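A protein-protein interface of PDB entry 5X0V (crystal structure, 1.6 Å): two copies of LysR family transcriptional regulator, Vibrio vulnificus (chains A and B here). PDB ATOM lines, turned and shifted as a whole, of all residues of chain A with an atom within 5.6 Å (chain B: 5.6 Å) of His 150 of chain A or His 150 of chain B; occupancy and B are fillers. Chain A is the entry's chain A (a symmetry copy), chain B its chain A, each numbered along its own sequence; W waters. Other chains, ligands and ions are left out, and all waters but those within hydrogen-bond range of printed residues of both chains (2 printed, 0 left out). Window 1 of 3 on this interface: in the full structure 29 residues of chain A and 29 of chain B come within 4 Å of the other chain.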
ATOM      1  N   ALA A  27      17.979  21.886 -19.297  1.00  0.00           N
ATOM      2  CA  ALA A  27      17.461  20.586 -18.859  1.00  0.00           C
ATOM      3  C   ALA A  27      16.371  20.006 -19.765  1.00  0.00           C
ATOM      4  O   ALA A  27      16.439  18.802 -20.088  1.00  0.00           O
ATOM      5  CB  ALA A  27      16.965  20.744 -17.411  1.00  0.00           C
ATOM      6  N   PRO A  28      15.364  20.761 -20.196  1.00  0.00           N
ATOM      7  CA  PRO A  28      14.290  20.143 -21.003  1.00  0.00           C
ATOM      8  C   PRO A  28      14.762  19.663 -22.336  1.00  0.00           C
ATOM      9  O   PRO A  28      13.998  18.956 -23.005  1.00  0.00           O
ATOM     10  CB  PRO A  28      13.306  21.287 -21.224  1.00  0.00           C
ATOM     11  CG  PRO A  28      13.588  22.284 -20.179  1.00  0.00           C
ATOM     12  CD  PRO A  28      15.081  22.199 -19.958  1.00  0.00           C
ATOM     13  N   PHE A  29      15.933  20.104 -22.796  1.00  0.00           N
ATOM     14  CA  PHE A  29      16.340  19.864 -24.183  1.00  0.00           C
ATOM     15  C   PHE A  29      17.422  18.782 -24.193  1.00  0.00           C
ATOM     16  O   PHE A  29      17.144  17.624 -24.545  1.00  0.00           O
ATOM     17  CB  PHE A  29      16.764  21.184 -24.821  1.00  0.00           C
ATOM     18  CG  PHE A  29      15.776  22.305 -24.529  1.00  0.00           C
ATOM     19  CD1 PHE A  29      14.434  22.224 -24.965  1.00  0.00           C
ATOM     20  CD2 PHE A  29      16.176  23.378 -23.762  1.00  0.00           C
ATOM     21  CE1 PHE A  29      13.542  23.191 -24.677  1.00  0.00           C
ATOM     22  CE2 PHE A  29      15.278  24.366 -23.436  1.00  0.00           C
ATOM     23  CZ  PHE A  29      13.934  24.285 -23.918  1.00  0.00           C
ATOM     24  N   GLU A  51      16.428  20.152 -11.394  1.00  0.00           N
ATOM     25  CA  GLU A  51      16.414  21.368 -12.212  1.00  0.00           C
ATOM     26  C   GLU A  51      16.280  22.577 -11.307  1.00  0.00           C
ATOM     27  O   GLU A  51      15.348  22.647 -10.489  1.00  0.00           O
ATOM     28  CB  GLU A  51      15.254  21.284 -13.214  1.00  0.00           C
ATOM     29  CG  GLU A  51      15.214  22.528 -14.143  1.00  0.00           C
ATOM     30  CD  GLU A  51      14.095  22.450 -15.227  1.00  0.00           C
ATOM     31  OE1 GLU A  51      13.405  23.479 -15.356  1.00  0.00           O
ATOM     32  OE2 GLU A  51      13.855  21.374 -15.860  1.00  0.00           O
ATOM     33  N   SER A 148      10.058  32.031 -17.431  1.00  0.00           N
ATOM     34  CA  SER A 148      10.413  30.724 -17.982  1.00  0.00           C
ATOM     35  C   SER A 148      10.647  30.871 -19.468  1.00  0.00           C
ATOM     36  O   SER A 148      10.114  31.778 -20.137  1.00  0.00           O
ATOM     37  CB  SER A 148       9.317  29.653 -17.719  1.00  0.00           C
ATOM     38  OG  SER A 148       8.194  29.871 -18.582  1.00  0.00           O
ATOM     39  N   LEU A 149      11.443  29.932 -19.999  1.00  0.00           N
ATOM     40  CA  LEU A 149      11.734  29.977 -21.406  1.00  0.00           C
ATOM     41  C   LEU A 149      10.462  29.756 -22.220  1.00  0.00           C
ATOM     42  O   LEU A 149      10.222  30.456 -23.199  1.00  0.00           O
ATOM     43  CB  LEU A 149      12.794  28.933 -21.716  1.00  0.00           C
ATOM     44  CG  LEU A 149      13.402  29.060 -23.088  1.00  0.00           C
ATOM     45  CD1 LEU A 149      13.977  30.426 -23.362  1.00  0.00           C
ATOM     46  CD2 LEU A 149      14.522  27.974 -23.124  1.00  0.00           C
ATOM     47  N   HIS A 150       9.572  28.890 -21.755  1.00  0.00           N
ATOM     48  CA  HIS A 150       8.337  28.626 -22.502  1.00  0.00           C
ATOM     49  C   HIS A 150       7.431  29.846 -22.586  1.00  0.00           C
ATOM     50  O   HIS A 150       6.829  30.099 -23.650  1.00  0.00           O
ATOM     51  CB  HIS A 150       7.535  27.478 -21.872  1.00  0.00           C
ATOM     52  CG  HIS A 150       8.350  26.260 -21.720  1.00  0.00           C
ATOM     53  ND1 HIS A 150       9.217  26.082 -20.656  1.00  0.00           N
ATOM     54  CD2 HIS A 150       8.532  25.210 -22.554  1.00  0.00           C
ATOM     55  CE1 HIS A 150       9.887  24.952 -20.843  1.00  0.00           C
ATOM     56  NE2 HIS A 150       9.487  24.410 -21.984  1.00  0.00           N
ATOM     57  N   THR A 151       7.247  30.562 -21.469  1.00  0.00           N
ATOM     58  CA  THR A 151       6.356  31.728 -21.453  1.00  0.00           C
ATOM     59  C   THR A 151       7.015  32.947 -22.103  1.00  0.00           C
ATOM     60  O   THR A 151       6.305  33.745 -22.735  1.00  0.00           O
ATOM     61  CB  THR A 151       5.875  32.058 -20.013  1.00  0.00           C
ATOM     62  OG1 THR A 151       7.002  32.264 -19.123  1.00  0.00           O
ATOM     63  CG2 THR A 151       4.871  30.943 -19.460  1.00  0.00           C
ATOM     64  N   LEU A 152       8.365  33.034 -22.073  1.00  0.00           N
ATOM     65  CA  LEU A 152       9.072  34.028 -22.874  1.00  0.00           C
ATOM     66  C   LEU A 152       8.720  33.867 -24.342  1.00  0.00           C
ATOM     67  O   LEU A 152       8.346  34.821 -25.030  1.00  0.00           O
ATOM     68  CB  LEU A 152      10.598  33.879 -22.668  1.00  0.00           C
ATOM     69  CG  LEU A 152      11.525  34.769 -23.479  1.00  0.00           C
ATOM     70  CD1 LEU A 152      11.171  36.241 -23.264  1.00  0.00           C
ATOM     71  CD2 LEU A 152      12.980  34.457 -23.029  1.00  0.00           C
ATOM     72  N   VAL A 153       8.842  32.637 -24.841  1.00  0.00           N
ATOM     73  CA  VAL A 153       8.562  32.378 -26.257  1.00  0.00           C
ATOM     74  C   VAL A 153       7.094  32.644 -26.593  1.00  0.00           C
ATOM     75  O   VAL A 153       6.768  33.138 -27.688  1.00  0.00           O
ATOM     76  CB  VAL A 153       8.966  30.931 -26.587  1.00  0.00           C
ATOM     77  CG1 VAL A 153       8.345  30.456 -27.941  1.00  0.00           C
ATOM     78  CG2 VAL A 153      10.498  30.835 -26.686  1.00  0.00           C
ATOM     79  N   GLN A 154       6.173  32.279 -25.678  1.00  0.00           N
ATOM     80  CA  GLN A 154       4.744  32.526 -25.902  1.00  0.00           C
ATOM     81  C   GLN A 154       4.464  34.011 -26.015  1.00  0.00           C
ATOM     82  O   GLN A 154       3.662  34.431 -26.860  1.00  0.00           O
ATOM     83  CB  GLN A 154       3.919  31.921 -24.764  1.00  0.00           C
ATOM     84  CG  GLN A 154       3.877  30.376 -24.839  1.00  0.00           C
ATOM     85  CD  GLN A 154       3.699  29.707 -23.514  1.00  0.00           C
ATOM     86  OE1 GLN A 154       3.567  30.371 -22.500  1.00  0.00           O
ATOM     87  NE2 GLN A 154       3.692  28.333 -23.505  1.00  0.00           N
ATOM     88  N   MET A 155       5.111  34.840 -25.185  1.00  0.00           N
ATOM     89  CA  MET A 155       4.902  36.280 -25.377  1.00  0.00           C
ATOM     90  C   MET A 155       5.378  36.738 -26.757  1.00  0.00           C
ATOM     91  O   MET A 155       4.770  37.627 -27.356  1.00  0.00           O
ATOM     92  CB  MET A 155       5.624  37.110 -24.299  1.00  0.00           C
ATOM     93  CG  MET A 155       4.920  36.955 -22.924  1.00  0.00           C
ATOM     94  SD  MET A 155       5.590  38.076 -21.686  1.00  0.00           S
ATOM     95  CE  MET A 155       7.161  37.253 -21.288  1.00  0.00           C
ATOM     96  N   LEU A 174      10.827  23.574 -29.347  1.00  0.00           N
ATOM     97  CA  LEU A 174      10.200  24.622 -28.540  1.00  0.00           C
ATOM     98  C   LEU A 174       9.312  25.563 -29.374  1.00  0.00           C
ATOM     99  O   LEU A 174       8.276  26.055 -28.880  1.00  0.00           O
ATOM    100  CB  LEU A 174      11.274  25.423 -27.780  1.00  0.00           C
ATOM    101  CG  LEU A 174      10.689  26.488 -26.845  1.00  0.00           C
ATOM    102  CD1 LEU A 174       9.856  25.869 -25.704  1.00  0.00           C
ATOM    103  CD2 LEU A 174      11.860  27.304 -26.235  1.00  0.00           C
ATOM    104  N   GLN A 178       3.991  27.605 -33.166  1.00  0.00           N
ATOM    105  CA  GLN A 178       3.797  28.935 -32.603  1.00  0.00           C
ATOM    106  C   GLN A 178       4.003  30.027 -33.634  1.00  0.00           C
ATOM    107  O   GLN A 178       4.023  31.199 -33.265  1.00  0.00           O
ATOM    108  CB  GLN A 178       4.725  29.155 -31.407  1.00  0.00           C
ATOM    109  CG  GLN A 178       4.436  28.063 -30.317  1.00  0.00           C
ATOM    110  CD  GLN A 178       4.922  28.513 -28.929  1.00  0.00           C
ATOM    111  OE1 GLN A 178       5.942  28.028 -28.415  1.00  0.00           O
ATOM    112  NE2 GLN A 178       4.239  29.490 -28.366  1.00  0.00           N
ATOM    113  N   ALA B  27       1.573  25.836 -18.014  1.00  0.00           N
ATOM    114  CA  ALA B  27       2.010  26.939 -18.877  1.00  0.00           C
ATOM    115  C   ALA B  27       2.680  26.490 -20.180  1.00  0.00           C
ATOM    116  O   ALA B  27       2.346  27.046 -21.246  1.00  0.00           O
ATOM    117  CB  ALA B  27       2.940  27.842 -18.048  1.00  0.00           C
ATOM    118  N   PRO B  28       3.603  25.533 -20.180  1.00  0.00           N
ATOM    119  CA  PRO B  28       4.283  25.185 -21.447  1.00  0.00           C
ATOM    120  C   PRO B  28       3.364  24.574 -22.454  1.00  0.00           C
ATOM    121  O   PRO B  28       3.782  24.431 -23.610  1.00  0.00           O
ATOM    122  CB  PRO B  28       5.304  24.134 -21.027  1.00  0.00           C
ATOM    123  CG  PRO B  28       5.499  24.299 -19.578  1.00  0.00           C
ATOM    124  CD  PRO B  28       4.146  24.730 -19.055  1.00  0.00           C
ATOM    125  N   PHE B  29       2.184  24.110 -22.045  1.00  0.00           N
ATOM    126  CA  PHE B  29       1.347  23.293 -22.925  1.00  0.00           C
ATOM    127  C   PHE B  29       0.170  24.146 -23.408  1.00  0.00           C
ATOM    128  O   PHE B  29       0.161  24.601 -24.562  1.00  0.00           O
ATOM    129  CB  PHE B  29       0.939  22.015 -22.195  1.00  0.00           C
ATOM    130  CG  PHE B  29       2.118  21.360 -21.488  1.00  0.00           C
ATOM    131  CD1 PHE B  29       3.238  20.900 -22.216  1.00  0.00           C
ATOM    132  CD2 PHE B  29       2.126  21.286 -20.112  1.00  0.00           C
ATOM    133  CE1 PHE B  29       4.303  20.355 -21.596  1.00  0.00           C
ATOM    134  CE2 PHE B  29       3.211  20.756 -19.456  1.00  0.00           C
ATOM    135  CZ  PHE B  29       4.319  20.259 -20.211  1.00  0.00           C
ATOM    136  N   GLU B  51       5.190  32.627 -15.067  1.00  0.00           N
ATOM    137  CA  GLU B  51       5.126  31.222 -14.654  1.00  0.00           C
ATOM    138  C   GLU B  51       5.698  31.086 -13.257  1.00  0.00           C
ATOM    139  O   GLU B  51       6.835  31.516 -13.001  1.00  0.00           O
ATOM    140  CB  GLU B  51       5.902  30.367 -15.667  1.00  0.00           C
ATOM    141  CG  GLU B  51       5.835  28.858 -15.307  1.00  0.00           C
ATOM    142  CD  GLU B  51       6.548  27.945 -16.350  1.00  0.00           C
ATOM    143  OE1 GLU B  51       7.305  27.079 -15.872  1.00  0.00           O
ATOM    144  OE2 GLU B  51       6.429  28.143 -17.601  1.00  0.00           O
ATOM    145  N   SER B 148      11.039  19.473 -11.766  1.00  0.00           N
ATOM    146  CA  SER B 148      10.352  19.967 -12.958  1.00  0.00           C
ATOM    147  C   SER B 148       9.700  18.799 -13.662  1.00  0.00           C
ATOM    148  O   SER B 148      10.127  17.634 -13.549  1.00  0.00           O
ATOM    149  CB  SER B 148      11.312  20.708 -13.930  1.00  0.00           C
ATOM    150  OG  SER B 148      12.139  19.765 -14.624  1.00  0.00           O
ATOM    151  N   LEU B 149       8.655  19.131 -14.435  1.00  0.00           N
ATOM    152  CA  LEU B 149       7.961  18.097 -15.151  1.00  0.00           C
ATOM    153  C   LEU B 149       8.881  17.456 -16.188  1.00  0.00           C
ATOM    154  O   LEU B 149       8.908  16.237 -16.322  1.00  0.00           O
ATOM    155  CB  LEU B 149       6.720  18.698 -15.790  1.00  0.00           C
ATOM    156  CG  LEU B 149       5.748  17.681 -16.329  1.00  0.00           C
ATOM    157  CD1 LEU B 149       5.317  16.667 -15.301  1.00  0.00           C
ATOM    158  CD2 LEU B 149       4.529  18.523 -16.817  1.00  0.00           C
ATOM    159  N   HIS B 150       9.737  18.241 -16.824  1.00  0.00           N
ATOM    160  CA  HIS B 150      10.638  17.684 -17.841  1.00  0.00           C
ATOM    161  C   HIS B 150      11.639  16.696 -17.259  1.00  0.00           C
ATOM    162  O   HIS B 150      11.918  15.654 -17.887  1.00  0.00           O
ATOM    163  CB  HIS B 150      11.422  18.789 -18.563  1.00  0.00           C
ATOM    164  CG  HIS B 150      10.528  19.813 -19.130  1.00  0.00           C
ATOM    165  ND1 HIS B 150      10.009  20.844 -18.365  1.00  0.00           N
ATOM    166  CD2 HIS B 150       9.954  19.906 -20.353  1.00  0.00           C
ATOM    167  CE1 HIS B 150       9.161  21.538 -19.114  1.00  0.00           C
ATOM    168  NE2 HIS B 150       9.114  20.986 -20.318  1.00  0.00           N
ATOM    169  N   THR B 151      12.253  17.033 -16.118  1.00  0.00           N
ATOM    170  CA  THR B 151      13.261  16.156 -15.511  1.00  0.00           C
ATOM    171  C   THR B 151      12.616  14.970 -14.792  1.00  0.00           C
ATOM    172  O   THR B 151      13.205  13.877 -14.790  1.00  0.00           O
ATOM    173  CB  THR B 151      14.199  16.943 -14.554  1.00  0.00           C
ATOM    174  OG1 THR B 151      13.438  17.630 -13.529  1.00  0.00           O
ATOM    175  CG2 THR B 151      15.155  17.941 -15.359  1.00  0.00           C
ATOM    176  N   LEU B 152      11.366  15.127 -14.299  1.00  0.00           N
ATOM    177  CA  LEU B 152      10.596  13.981 -13.822  1.00  0.00           C
ATOM    178  C   LEU B 152      10.460  12.945 -14.923  1.00  0.00           C
ATOM    179  O   LEU B 152      10.738  11.757 -14.737  1.00  0.00           O
ATOM    180  CB  LEU B 152       9.201  14.448 -13.346  1.00  0.00           C
ATOM    181  CG  LEU B 152       8.206  13.394 -12.886  1.00  0.00           C
ATOM    182  CD1 LEU B 152       8.813  12.542 -11.771  1.00  0.00           C
ATOM    183  CD2 LEU B 152       6.929  14.139 -12.408  1.00  0.00           C
ATOM    184  N   VAL B 153      10.019  13.395 -16.098  1.00  0.00           N
ATOM    185  CA  VAL B 153       9.816  12.472 -17.219  1.00  0.00           C
ATOM    186  C   VAL B 153      11.134  11.840 -17.667  1.00  0.00           C
ATOM    187  O   VAL B 153      11.179  10.657 -18.052  1.00  0.00           O
ATOM    188  CB  VAL B 153       9.130  13.229 -18.370  1.00  0.00           C
ATOM    189  CG1 VAL B 153       9.236  12.445 -19.717  1.00  0.00           C
ATOM    190  CG2 VAL B 153       7.642  13.435 -18.033  1.00  0.00           C
ATOM    191  N   GLN B 154      12.228  12.628 -17.674  1.00  0.00           N
ATOM    192  CA  GLN B 154      13.542  12.098 -18.058  1.00  0.00           C
ATOM    193  C   GLN B 154      13.982  11.004 -17.106  1.00  0.00           C
ATOM    194  O   GLN B 154      14.539   9.988 -17.541  1.00  0.00           O
ATOM    195  CB  GLN B 154      14.579  13.223 -18.080  1.00  0.00           C
ATOM    196  CG  GLN B 154      14.377  14.170 -19.287  1.00  0.00           C
ATOM    197  CD  GLN B 154      14.852  15.568 -19.049  1.00  0.00           C
ATOM    198  OE1 GLN B 154      15.378  15.869 -17.991  1.00  0.00           O
ATOM    199  NE2 GLN B 154      14.667  16.471 -20.067  1.00  0.00           N
ATOM    200  N   MET B 155      13.741  11.171 -15.799  1.00  0.00           N
ATOM    201  CA  MET B 155      14.084  10.058 -14.905  1.00  0.00           C
ATOM    202  C   MET B 155      13.282   8.800 -15.242  1.00  0.00           C
ATOM    203  O   MET B 155      13.798   7.687 -15.123  1.00  0.00           O
ATOM    204  CB  MET B 155      13.850  10.419 -13.427  1.00  0.00           C
ATOM    205  CG  MET B 155      14.907  11.443 -12.937  1.00  0.00           C
ATOM    206  SD  MET B 155      14.811  11.726 -11.162  1.00  0.00           S
ATOM    207  CE  MET B 155      13.336  12.782 -11.060  1.00  0.00           C
ATOM    208  N   LEU B 174       5.496  16.248 -24.917  1.00  0.00           N
ATOM    209  CA  LEU B 174       6.480  16.074 -23.848  1.00  0.00           C
ATOM    210  C   LEU B 174       7.197  14.713 -23.915  1.00  0.00           C
ATOM    211  O   LEU B 174       8.393  14.613 -23.570  1.00  0.00           O
ATOM    212  CB  LEU B 174       5.813  16.268 -22.474  1.00  0.00           C
ATOM    213  CG  LEU B 174       6.799  16.185 -21.302  1.00  0.00           C
ATOM    214  CD1 LEU B 174       7.844  17.320 -21.336  1.00  0.00           C
ATOM    215  CD2 LEU B 174       5.997  16.271 -19.977  1.00  0.00           C
ATOM    216  N   GLN B 178      11.348   9.806 -26.273  1.00  0.00           N
ATOM    217  CA  GLN B 178      11.889   9.328 -25.007  1.00  0.00           C
ATOM    218  C   GLN B 178      11.536   7.877 -24.746  1.00  0.00           C
ATOM    219  O   GLN B 178      11.796   7.388 -23.649  1.00  0.00           O
ATOM    220  CB  GLN B 178      11.411  10.205 -23.849  1.00  0.00           C
ATOM    221  CG  GLN B 178      11.858  11.688 -24.099  1.00  0.00           C
ATOM    222  CD  GLN B 178      11.886  12.495 -22.791  1.00  0.00           C
ATOM    223  OE1 GLN B 178      11.013  13.338 -22.535  1.00  0.00           O
ATOM    224  NE2 GLN B 178      12.839  12.178 -21.936  1.00  0.00           N
HETATM  225  O   HOH W   1       8.746  25.824 -17.809  1.00  0.00           O
HETATM  226  O   HOH W   2      11.281  23.062 -17.005  1.00  0.00           O
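O of His 150 of chain B lies close to OE1 of Gln 154 of chain B, 3.5 Å away.
O of His 150 of chain A sits close to OE1 of Gln 154 of chain A.
The side-chain hydroxyl (OG) of Ser 148 of chain B is in hydrogen-bond range of the side-chain hydroxyl (OG1) of Thr 151 of chain B, at 2.7 Å.
OG1 of Thr 151 of chain A is in hydrogen-bond range of OG of Ser 148 of chain A (2.7 Å).
Of the printed residues of chain B, Pro 28 of chain A touches His 150 and Gln 154.
His 150 of chain A touches two residues of chain B.
Of the printed residues of chain A, Ala 27 of chain B touches Thr 151 (3.9 Å) and Gln 154 (2.9 Å).
Printed residues of chain A within 4 Å of Ser 148 of chain B: Glu 51 (2.7 Å).
Leu 149 of chain B touches none of the printed residues of chain A.
Of chain A, only Pro 28 and His 150 come within 4 Å of His 150 of chain B.
Of the printed residues of chain A, Gln 154 of chain B touches Ala 27 (2.9 Å) and Pro 28 (3.8 Å).
The nearest residue of chain B that does not touch His 150 of chain A is Glu 51 of chain B (4.5 Å).
Of the 14 printed residues of chain B, 7 touch a printed residue of chain A.
Printed residues of chain B that touch a printed residue of chain A: Ala 27, Pro 28, Glu 51, Ser 148, His 150, Thr 151 and Gln 154.
Hydrophobic or aromatic side chains of chain B within 4 Å of the printed part of chain A: Ala 27, Pro 28 and His 150.
Along chain B the printed residues that touch a printed residue of chain A span positions 27 to 154.
Among the printed residues, no Asp or Glu carboxylate lies within 4 Å of a Lys or Arg side-chain nitrogen of the other chain.
OE2 of Glu 51 of chain B is in hydrogen-bond range of OG of Ser 148 of chain A, at 2.7 Å.
The side-chain amide nitrogen (NE2) of Gln 154 of chain B lies within hydrogen-bond range of the backbone carbonyl oxygen (O) of Ala 27 of chain A, at 2.9 Å.
O of Ala 27 of chain B is in hydrogen-bond range of NE2 of Gln 154 of chain A (2.9 Å).
The side-chain carboxylate (OE2) of Glu 51 of chain A lies within hydrogen-bond range of the side-chain hydroxyl (OG) of Ser 148 of chain B.
Among the printed residues, merely in contact across the chains: Thr 151 of chain A with Glu 51 of chain B, Glu 51 of chain A with Thr 151 of chain B, Pro 28 of chain A with His 150 of chain B, His 150 of chain A with Pro 28 of chain B, Gln 154 of chain A with Pro 28 of chain B, Pro 28 of chain A with Gln 154 of chain B, His 150 of chain A with His 150 of chain B, Thr 151 of chain A with Ala 27 of chain B and Ala 27 of chain A with Thr 151 of chain B.
Ala 27 of chain A touches Thr 151 of chain B, and with the chains exchanged Thr 151 of chain A touches Ala 27 of chain B.
Pro 28 of chain A touches His 150 of chain B, and with the chains exchanged His 150 of chain A touches Pro 28 of chain B.
Glu 51 of chain A touches Ser 148 of chain B, and with the chains exchanged Ser 148 of chain A touches Glu 51 of chain B.
His 150 of chain B touches its own counterpart, His 150 of chain A.
Water W1 lies within hydrogen-bond range of OE1 of Glu 51 of chain B (2.7 Å) and ND1 of His 150 of chain A (2.9 Å).
Water W2 lies within hydrogen-bond range of OE1 of Glu 51 of chain A (2.7 Å) and ND1 of His 150 of chain B (2.9 Å).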
